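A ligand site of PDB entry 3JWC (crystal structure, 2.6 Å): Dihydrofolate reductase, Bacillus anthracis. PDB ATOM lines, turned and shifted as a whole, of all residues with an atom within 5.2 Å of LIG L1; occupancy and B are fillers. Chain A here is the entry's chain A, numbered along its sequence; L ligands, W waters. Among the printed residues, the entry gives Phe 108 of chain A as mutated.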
ATOM      1  N   MET A  12       4.528   8.279  24.417  1.00  0.00           N
ATOM      2  CA  MET A  12       3.299   7.895  23.751  1.00  0.00           C
ATOM      3  C   MET A  12       3.405   8.401  22.322  1.00  0.00           C
ATOM      4  O   MET A  12       3.476   9.602  22.071  1.00  0.00           O
ATOM      5  CB  MET A  12       2.095   8.503  24.466  1.00  0.00           C
ATOM      6  CG  MET A  12       0.761   8.342  23.731  1.00  0.00           C
ATOM      7  SD  MET A  12       0.190   6.634  23.459  1.00  0.00           S
ATOM      8  CE  MET A  12      -0.091   6.054  25.134  1.00  0.00           C
ATOM      9  N   VAL A  13       3.430   7.455  21.373  1.00  0.00           N
ATOM     10  CA  VAL A  13       3.667   7.796  19.979  1.00  0.00           C
ATOM     11  C   VAL A  13       3.018   6.808  18.994  1.00  0.00           C
ATOM     12  O   VAL A  13       2.943   5.607  19.269  1.00  0.00           O
ATOM     13  CB  VAL A  13       5.187   7.995  19.709  1.00  0.00           C
ATOM     14  CG1 VAL A  13       5.949   6.680  19.836  1.00  0.00           C
ATOM     15  CG2 VAL A  13       5.420   8.636  18.348  1.00  0.00           C
ATOM     16  N   ALA A  14       2.543   7.341  17.866  1.00  0.00           N
ATOM     17  CA  ALA A  14       2.096   6.547  16.724  1.00  0.00           C
ATOM     18  C   ALA A  14       2.947   6.896  15.501  1.00  0.00           C
ATOM     19  O   ALA A  14       3.079   8.066  15.147  1.00  0.00           O
ATOM     20  CB  ALA A  14       0.638   6.793  16.437  1.00  0.00           C
ATOM     21  N   ASN A  25       2.748  20.057   9.836  1.00  0.00           N
ATOM     22  CA  ASN A  25       2.392  20.410  11.213  1.00  0.00           C
ATOM     23  C   ASN A  25       1.043  19.806  11.678  1.00  0.00           C
ATOM     24  O   ASN A  25       0.332  20.381  12.508  1.00  0.00           O
ATOM     25  CB  ASN A  25       2.459  21.929  11.428  1.00  0.00           C
ATOM     26  CG  ASN A  25       2.668  22.307  12.875  1.00  0.00           C
ATOM     27  OD1 ASN A  25       3.318  21.595  13.647  1.00  0.00           O
ATOM     28  ND2 ASN A  25       2.121  23.458  13.269  1.00  0.00           N
ATOM     29  N   ASN A  26       0.721  18.635  11.124  1.00  0.00           N
ATOM     30  CA  ASN A  26      -0.489  17.889  11.475  1.00  0.00           C
ATOM     31  C   ASN A  26      -0.214  16.375  11.452  1.00  0.00           C
ATOM     32  O   ASN A  26       0.891  15.938  11.108  1.00  0.00           O
ATOM     33  CB  ASN A  26      -1.622  18.244  10.508  1.00  0.00           C
ATOM     34  CG  ASN A  26      -3.028  18.088  11.120  1.00  0.00           C
ATOM     35  OD1 ASN A  26      -3.213  17.475  12.190  1.00  0.00           O
ATOM     36  ND2 ASN A  26      -4.021  18.649  10.446  1.00  0.00           N
ATOM     37  N   LEU A  27      -1.234  15.600  11.828  1.00  0.00           N
ATOM     38  CA  LEU A  27      -1.227  14.152  11.702  1.00  0.00           C
ATOM     39  C   LEU A  27      -1.459  13.734  10.251  1.00  0.00           C
ATOM     40  O   LEU A  27      -2.285  14.342   9.551  1.00  0.00           O
ATOM     41  CB  LEU A  27      -2.331  13.556  12.581  1.00  0.00           C
ATOM     42  CG  LEU A  27      -2.028  13.156  14.042  1.00  0.00           C
ATOM     43  CD1 LEU A  27      -0.876  13.923  14.691  1.00  0.00           C
ATOM     44  CD2 LEU A  27      -3.298  13.273  14.886  1.00  0.00           C
ATOM     45  N   TRP A  29      -2.698  10.825   9.275  1.00  0.00           N
ATOM     46  CA  TRP A  29      -3.752   9.819   9.171  1.00  0.00           C
ATOM     47  C   TRP A  29      -4.870  10.116  10.153  1.00  0.00           C
ATOM     48  O   TRP A  29      -4.666  10.813  11.150  1.00  0.00           O
ATOM     49  CB  TRP A  29      -3.179   8.420   9.459  1.00  0.00           C
ATOM     50  CG  TRP A  29      -2.449   8.369  10.762  1.00  0.00           C
ATOM     51  CD1 TRP A  29      -3.000   8.306  12.004  1.00  0.00           C
ATOM     52  CD2 TRP A  29      -1.028   8.415  10.956  1.00  0.00           C
ATOM     53  NE1 TRP A  29      -2.023   8.306  12.960  1.00  0.00           N
ATOM     54  CE2 TRP A  29      -0.796   8.370  12.339  1.00  0.00           C
ATOM     55  CE3 TRP A  29       0.067   8.483  10.088  1.00  0.00           C
ATOM     56  CZ2 TRP A  29       0.502   8.386  12.896  1.00  0.00           C
ATOM     57  CZ3 TRP A  29       1.370   8.495  10.638  1.00  0.00           C
ATOM     58  CH2 TRP A  29       1.564   8.451  12.022  1.00  0.00           C
ATOM     59  N   GLU A  34      -7.471   4.629  17.564  1.00  0.00           N
ATOM     60  CA  GLU A  34      -6.136   4.787  18.107  1.00  0.00           C
ATOM     61  C   GLU A  34      -6.128   5.977  19.068  1.00  0.00           C
ATOM     62  O   GLU A  34      -5.479   5.924  20.123  1.00  0.00           O
ATOM     63  CB  GLU A  34      -5.132   4.978  16.957  1.00  0.00           C
ATOM     64  CG  GLU A  34      -3.707   4.488  17.231  1.00  0.00           C
ATOM     65  CD  GLU A  34      -2.833   5.491  18.002  1.00  0.00           C
ATOM     66  OE1 GLU A  34      -2.998   6.720  17.792  1.00  0.00           O
ATOM     67  OE2 GLU A  34      -1.984   5.050  18.815  1.00  0.00           O
ATOM     68  N   LEU A  35      -6.859   7.036  18.716  1.00  0.00           N
ATOM     69  CA  LEU A  35      -7.117   8.164  19.618  1.00  0.00           C
ATOM     70  C   LEU A  35      -7.771   7.729  20.924  1.00  0.00           C
ATOM     71  O   LEU A  35      -7.420   8.234  21.984  1.00  0.00           O
ATOM     72  CB  LEU A  35      -8.034   9.161  18.956  1.00  0.00           C
ATOM     73  CG  LEU A  35      -7.523  10.550  18.609  1.00  0.00           C
ATOM     74  CD1 LEU A  35      -6.499  10.468  17.473  1.00  0.00           C
ATOM     75  CD2 LEU A  35      -8.738  11.420  18.241  1.00  0.00           C
ATOM     76  N   VAL A  38      -5.227   6.038  23.038  1.00  0.00           N
ATOM     77  CA  VAL A  38      -4.396   7.114  23.578  1.00  0.00           C
ATOM     78  C   VAL A  38      -5.061   7.802  24.781  1.00  0.00           C
ATOM     79  O   VAL A  38      -4.417   7.981  25.816  1.00  0.00           O
ATOM     80  CB  VAL A  38      -4.024   8.145  22.484  1.00  0.00           C
ATOM     81  CG1 VAL A  38      -3.381   9.368  23.087  1.00  0.00           C
ATOM     82  CG2 VAL A  38      -3.079   7.518  21.476  1.00  0.00           C
ATOM     83  N   ASN A  53       3.450  20.924  18.832  1.00  0.00           N
ATOM     84  CA  ASN A  53       2.471  19.867  19.037  1.00  0.00           C
ATOM     85  C   ASN A  53       1.222  20.480  19.676  1.00  0.00           C
ATOM     86  O   ASN A  53       0.127  20.287  19.156  1.00  0.00           O
ATOM     87  CB  ASN A  53       3.050  18.725  19.893  1.00  0.00           C
ATOM     88  CG  ASN A  53       2.058  17.584  20.131  1.00  0.00           C
ATOM     89  OD1 ASN A  53       1.115  17.381  19.362  1.00  0.00           O
ATOM     90  ND2 ASN A  53       2.267  16.823  21.212  1.00  0.00           N
ATOM     91  N   ALA A  56      -1.237  22.896  17.431  1.00  0.00           N
ATOM     92  CA  ALA A  56      -2.003  22.113  16.463  1.00  0.00           C
ATOM     93  C   ALA A  56      -3.219  21.445  17.118  1.00  0.00           C
ATOM     94  O   ALA A  56      -4.300  21.393  16.514  1.00  0.00           O
ATOM     95  CB  ALA A  56      -1.108  21.078  15.789  1.00  0.00           C
ATOM     96  N   ILE A  57      -3.044  20.938  18.340  1.00  0.00           N
ATOM     97  CA  ILE A  57      -4.147  20.358  19.098  1.00  0.00           C
ATOM     98  C   ILE A  57      -5.193  21.437  19.416  1.00  0.00           C
ATOM     99  O   ILE A  57      -6.383  21.230  19.186  1.00  0.00           O
ATOM    100  CB  ILE A  57      -3.662  19.626  20.380  1.00  0.00           C
ATOM    101  CG1 ILE A  57      -2.889  18.364  20.008  1.00  0.00           C
ATOM    102  CG2 ILE A  57      -4.846  19.285  21.311  1.00  0.00           C
ATOM    103  CD1 ILE A  57      -2.103  17.762  21.162  1.00  0.00           C
ATOM    104  N   LEU A  61      -6.231  19.255  26.945  1.00  0.00           N
ATOM    105  CA  LEU A  61      -6.855  17.953  26.935  1.00  0.00           C
ATOM    106  C   LEU A  61      -7.379  17.596  28.335  1.00  0.00           C
ATOM    107  O   LEU A  61      -6.617  17.604  29.302  1.00  0.00           O
ATOM    108  CB  LEU A  61      -5.852  16.913  26.437  1.00  0.00           C
ATOM    109  CG  LEU A  61      -5.707  16.865  24.918  1.00  0.00           C
ATOM    110  CD1 LEU A  61      -4.251  16.879  24.490  1.00  0.00           C
ATOM    111  CD2 LEU A  61      -6.414  15.645  24.352  1.00  0.00           C
ATOM    112  N   PHE A 102       4.454  13.280  24.824  1.00  0.00           N
ATOM    113  CA  PHE A 102       3.374  13.190  23.871  1.00  0.00           C
ATOM    114  C   PHE A 102       3.749  13.736  22.478  1.00  0.00           C
ATOM    115  O   PHE A 102       2.942  13.694  21.558  1.00  0.00           O
ATOM    116  CB  PHE A 102       2.158  13.926  24.452  1.00  0.00           C
ATOM    117  CG  PHE A 102       0.842  13.542  23.822  1.00  0.00           C
ATOM    118  CD1 PHE A 102       0.334  12.242  23.960  1.00  0.00           C
ATOM    119  CD2 PHE A 102       0.092  14.473  23.112  1.00  0.00           C
ATOM    120  CE1 PHE A 102      -0.884  11.882  23.383  1.00  0.00           C
ATOM    121  CE2 PHE A 102      -1.123  14.122  22.531  1.00  0.00           C
ATOM    122  CZ  PHE A 102      -1.609  12.818  22.673  1.00  0.00           C
ATOM    123  N   GLY A 103       4.990  14.242  22.336  1.00  0.00           N
ATOM    124  CA  GLY A 103       5.486  14.736  21.048  1.00  0.00           C
ATOM    125  C   GLY A 103       5.550  16.249  20.904  1.00  0.00           C
ATOM    126  O   GLY A 103       5.198  16.982  21.822  1.00  0.00           O
ATOM    127  N   PHE A 108      10.374  14.637  21.536  1.00  0.00           N
ATOM    128  CA  PHE A 108      10.798  13.237  21.653  1.00  0.00           C
ATOM    129  C   PHE A 108      12.315  13.120  21.757  1.00  0.00           C
ATOM    130  O   PHE A 108      12.807  12.357  22.578  1.00  0.00           O
ATOM    131  CB  PHE A 108      10.281  12.357  20.520  1.00  0.00           C
ATOM    132  CG  PHE A 108       8.815  12.014  20.605  1.00  0.00           C
ATOM    133  CD1 PHE A 108       8.007  12.089  19.481  1.00  0.00           C
ATOM    134  CD2 PHE A 108       8.237  11.610  21.804  1.00  0.00           C
ATOM    135  CE1 PHE A 108       6.660  11.782  19.555  1.00  0.00           C
ATOM    136  CE2 PHE A 108       6.889  11.303  21.878  1.00  0.00           C
ATOM    137  CZ  PHE A 108       6.106  11.382  20.755  1.00  0.00           C
ATOM    138  N   TYR A 119       5.098   3.416  24.733  1.00  0.00           N
ATOM    139  CA  TYR A 119       3.817   3.009  24.157  1.00  0.00           C
ATOM    140  C   TYR A 119       3.784   3.475  22.714  1.00  0.00           C
ATOM    141  O   TYR A 119       3.531   4.670  22.437  1.00  0.00           O
ATOM    142  CB  TYR A 119       2.638   3.635  24.906  1.00  0.00           C
ATOM    143  CG  TYR A 119       2.583   3.366  26.392  1.00  0.00           C
ATOM    144  CD1 TYR A 119       3.467   3.981  27.276  1.00  0.00           C
ATOM    145  CD2 TYR A 119       1.609   2.530  26.925  1.00  0.00           C
ATOM    146  CE1 TYR A 119       3.402   3.741  28.639  1.00  0.00           C
ATOM    147  CE2 TYR A 119       1.538   2.277  28.279  1.00  0.00           C
ATOM    148  CZ  TYR A 119       2.435   2.895  29.127  1.00  0.00           C
ATOM    149  OH  TYR A 119       2.375   2.650  30.483  1.00  0.00           O
ATOM    150  N   THR A 121       2.467   2.880  18.743  1.00  0.00           N
ATOM    151  CA  THR A 121       1.601   2.310  17.716  1.00  0.00           C
ATOM    152  C   THR A 121       2.323   2.294  16.369  1.00  0.00           C
ATOM    153  O   THR A 121       2.800   3.324  15.903  1.00  0.00           O
ATOM    154  CB  THR A 121       0.281   3.095  17.596  1.00  0.00           C
ATOM    155  OG1 THR A 121      -0.326   3.209  18.888  1.00  0.00           O
ATOM    156  CG2 THR A 121      -0.692   2.401  16.647  1.00  0.00           C
HETATM  157  N1  LIG L   1       0.676   8.836  20.375  1.00  0.00           N
HETATM  158  C1  LIG L   1      -0.157   8.012  19.707  1.00  0.00           C
HETATM  159  N2  LIG L   1      -1.066   8.504  18.860  1.00  0.00           N
HETATM  160  C2  LIG L   1      -1.193   9.816  18.634  1.00  0.00           C
HETATM  161  C3  LIG L   1      -0.334  10.683  19.318  1.00  0.00           C
HETATM  162  C4  LIG L   1       0.606  10.164  20.205  1.00  0.00           C
HETATM  163  C5  LIG L   1      -1.748  10.081  16.227  1.00  0.00           C
HETATM  164  C6  LIG L   1      -3.140  17.937  15.457  1.00  0.00           C
HETATM  165  C7  LIG L   1      -5.194  14.119  21.096  1.00  0.00           C
HETATM  166  C8  LIG L   1      -6.873  15.244  16.740  1.00  0.00           C
HETATM  167  N3  LIG L   1      -0.111   6.702  19.875  1.00  0.00           N
HETATM  168  N4  LIG L   1       1.441  10.979  20.853  1.00  0.00           N
HETATM  169  C9  LIG L   1      -0.560  13.302  18.875  1.00  0.00           C
HETATM  170  C10 LIG L   1      -0.436  12.102  19.094  1.00  0.00           C
HETATM  171  C11 LIG L   1      -2.534  15.967  17.286  1.00  0.00           C
HETATM  172  C12 LIG L   1      -3.211  14.627  19.164  1.00  0.00           C
HETATM  173  C13 LIG L   1      -2.274  10.235  17.647  1.00  0.00           C
HETATM  174  C14 LIG L   1      -0.730  14.739  18.592  1.00  0.00           C
HETATM  175  O1  LIG L   1      -4.213  17.155  16.010  1.00  0.00           O
HETATM  176  O2  LIG L   1      -5.565  14.487  19.747  1.00  0.00           O
HETATM  177  O3  LIG L   1      -6.186  16.153  17.652  1.00  0.00           O
HETATM  178  C15 LIG L   1      -2.209  15.120  18.338  1.00  0.00           C
HETATM  179  C16 LIG L   1      -3.866  16.329  17.050  1.00  0.00           C
HETATM  180  C17 LIG L   1      -4.557  14.968  18.947  1.00  0.00           C
HETATM  181  C18 LIG L   1      -4.869  15.814  17.876  1.00  0.00           C
HETATM  182  P1  LG2 L   2       7.310  19.883  18.680  1.00  0.00           P
HETATM  183  O1  LG2 L   2       8.462  19.066  19.121  1.00  0.00           O
HETATM  184  O2  LG2 L   2       6.021  19.272  19.094  1.00  0.00           O
HETATM  185  O3  LG2 L   2       7.451  21.388  19.205  1.00  0.00           O
HETATM  186  C1  LG2 L   2       8.650  22.040  18.868  1.00  0.00           C
HETATM  187  C2  LG2 L   2       8.812  23.194  19.835  1.00  0.00           C
HETATM  188  O4  LG2 L   2       9.160  22.740  21.128  1.00  0.00           O
HETATM  189  C3  LG2 L   2       9.911  24.162  19.440  1.00  0.00           C
HETATM  190  O5  LG2 L   2       9.475  25.054  18.460  1.00  0.00           O
HETATM  191  C4  LG2 L   2      10.158  24.832  20.775  1.00  0.00           C
HETATM  192  O6  LG2 L   2       9.140  25.774  21.064  1.00  0.00           O
HETATM  193  C5  LG2 L   2       9.975  23.689  21.755  1.00  0.00           C
HETATM  194  N1  LG2 L   2      11.307  23.122  22.072  1.00  0.00           N
HETATM  195  C6  LG2 L   2      12.058  22.301  21.280  1.00  0.00           C
HETATM  196  N2  LG2 L   2      13.211  22.029  21.928  1.00  0.00           N
HETATM  197  C7  LG2 L   2      13.212  22.678  23.106  1.00  0.00           C
HETATM  198  C8  LG2 L   2      14.132  22.744  24.145  1.00  0.00           C
HETATM  199  N3  LG2 L   2      15.277  22.083  24.048  1.00  0.00           N
HETATM  200  N4  LG2 L   2      13.863  23.496  25.275  1.00  0.00           N
HETATM  201  C9  LG2 L   2      12.674  24.182  25.366  1.00  0.00           C
HETATM  202  N5  LG2 L   2      11.766  24.111  24.327  1.00  0.00           N
HETATM  203  C10 LG2 L   2      12.020  23.373  23.218  1.00  0.00           C
HETATM  204  O7  LG2 L   2       7.371  20.133  17.099  1.00  0.00           O
HETATM  205  P2  LG2 L   2       7.720  19.131  15.900  1.00  0.00           P
HETATM  206  O8  LG2 L   2       7.618  19.921  14.651  1.00  0.00           O
HETATM  207  O9  LG2 L   2       8.971  18.429  16.291  1.00  0.00           O
HETATM  208  O10 LG2 L   2       6.496  18.075  15.947  1.00  0.00           O
HETATM  209  C11 LG2 L   2       5.218  18.445  15.480  1.00  0.00           C
HETATM  210  C12 LG2 L   2       4.725  17.441  14.447  1.00  0.00           C
HETATM  211  O11 LG2 L   2       4.665  16.128  14.974  1.00  0.00           O
HETATM  212  C13 LG2 L   2       3.310  17.784  14.000  1.00  0.00           C
HETATM  213  O12 LG2 L   2       3.226  17.412  12.636  1.00  0.00           O
HETATM  214  C14 LG2 L   2       2.446  16.879  14.876  1.00  0.00           C
HETATM  215  O13 LG2 L   2       1.208  16.631  14.280  1.00  0.00           O
HETATM  216  C15 LG2 L   2       3.328  15.649  14.975  1.00  0.00           C
HETATM  217  N6  LG2 L   2       3.099  14.789  16.152  1.00  0.00           N
HETATM  218  C16 LG2 L   2       2.894  13.450  15.930  1.00  0.00           C
HETATM  219  C17 LG2 L   2       2.689  12.583  17.003  1.00  0.00           C
HETATM  220  C18 LG2 L   2       2.372  11.139  16.745  1.00  0.00           C
HETATM  221  O14 LG2 L   2       2.600  10.201  17.777  1.00  0.00           O
HETATM  222  N7  LG2 L   2       1.918  10.762  15.558  1.00  0.00           N
HETATM  223  C19 LG2 L   2       2.719  13.072  18.307  1.00  0.00           C
HETATM  224  C20 LG2 L   2       2.941  14.437  18.524  1.00  0.00           C
HETATM  225  C21 LG2 L   2       3.124  15.292  17.430  1.00  0.00           C
HETATM  226  P3  LG2 L   2       9.282  27.358  20.830  1.00  0.00           P
HETATM  227  O15 LG2 L   2      10.461  27.929  21.573  1.00  0.00           O
HETATM  228  O16 LG2 L   2       9.443  27.584  19.349  1.00  0.00           O
HETATM  229  O17 LG2 L   2       8.020  27.996  21.333  1.00  0.00           O
HETATM  230  O   HOH W   1      -3.708   7.896  15.184  1.00  0.00           O
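O2 of LG2 L2 lies within hydrogen-bond range of N of Asn 53 (3.1 Å).
The side-chain sulfur (SD) of Met 12 sits at hydrogen-bond distance from a nitrogen (N3) of LIG L1, 3.6 Å away.
OE2 of Glu 34 lies within hydrogen-bond range of N3 of LIG L1, 2.7 Å away.
O of Ala 14 sits at hydrogen-bond distance from N7 of LG2 L2, at 3.0 Å.
O14 of LG2 L2 is in hydrogen-bond range of N of Ala 14, at 2.9 Å.
The backbone carbonyl oxygen of Met 12 lies within hydrogen-bond range of a nitrogen (N4) of LIG L1, 2.7 Å away.
A nitrogen (N4) of LIG L1 sits at hydrogen-bond distance from the backbone carbonyl oxygen (O) of Phe 102.
The backbone carbonyl oxygen of Val 13 sits close to a nitrogen (N3) of LIG L1, 3.3 Å away.
O12 of LG2 L2 lies within hydrogen-bond range of N of Asn 26, 3.2 Å away.
A nitrogen (N1) of LIG L1 sits close to the backbone NH of Val 13, at 3.2 Å.
The backbone carbonyl oxygen of Asn 26 is in hydrogen-bond range of an oxygen (O12) of LG2 L2 (3.2 Å).
N1 of LIG L1 sits close to N of Ala 14 (3.5 Å).
N4 of LIG L1 sits close to O14 of LG2 L2 (3.4 Å).
The side-chain amide nitrogen (ND2) of Asn 53 is in hydrogen-bond range of the backbone carbonyl oxygen (O) of Phe 102.
N of Val 13 is in hydrogen-bond range of O of Tyr 119 (3.0 Å).
OE2 of Glu 34 sits at hydrogen-bond distance from OG1 of Thr 121, at 2.5 Å.
ND2 of Asn 53 is in hydrogen-bond range of O of Gly 103.
O of Val 13 is in hydrogen-bond range of N of Thr 121, 2.8 Å away.
Residues that only touch LIG L1: Asn 26 (3.3 Å), Asn 53 (3.3 Å), Val 38 (3.4 Å), Thr 121 (3.6 Å), Ile 57 (3.6 Å), Leu 27 (3.7 Å), Trp 29 (3.7 Å), Ala 56 (3.8 Å) and Leu 61 (3.8 Å).
Hydrophobic or aromatic side chains within 4 Å of LIG L1: Met 12, Ala 14, Leu 27, Val 38, Ala 56, Ile 57, Leu 61 and Phe 102.
14 residues have an atom within 4 Å of LIG L1: Met 12, Val 13, Ala 14, Asn 26, Leu 27, Trp 29, Glu 34, Val 38, Asn 53, Ala 56, Ile 57, Leu 61, Phe 102 and Thr 121.
Water W1 bridges the indole nitrogen of Trp 29 (2.8 Å) and the side-chain carboxylate of Glu 34 (2.9 Å).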
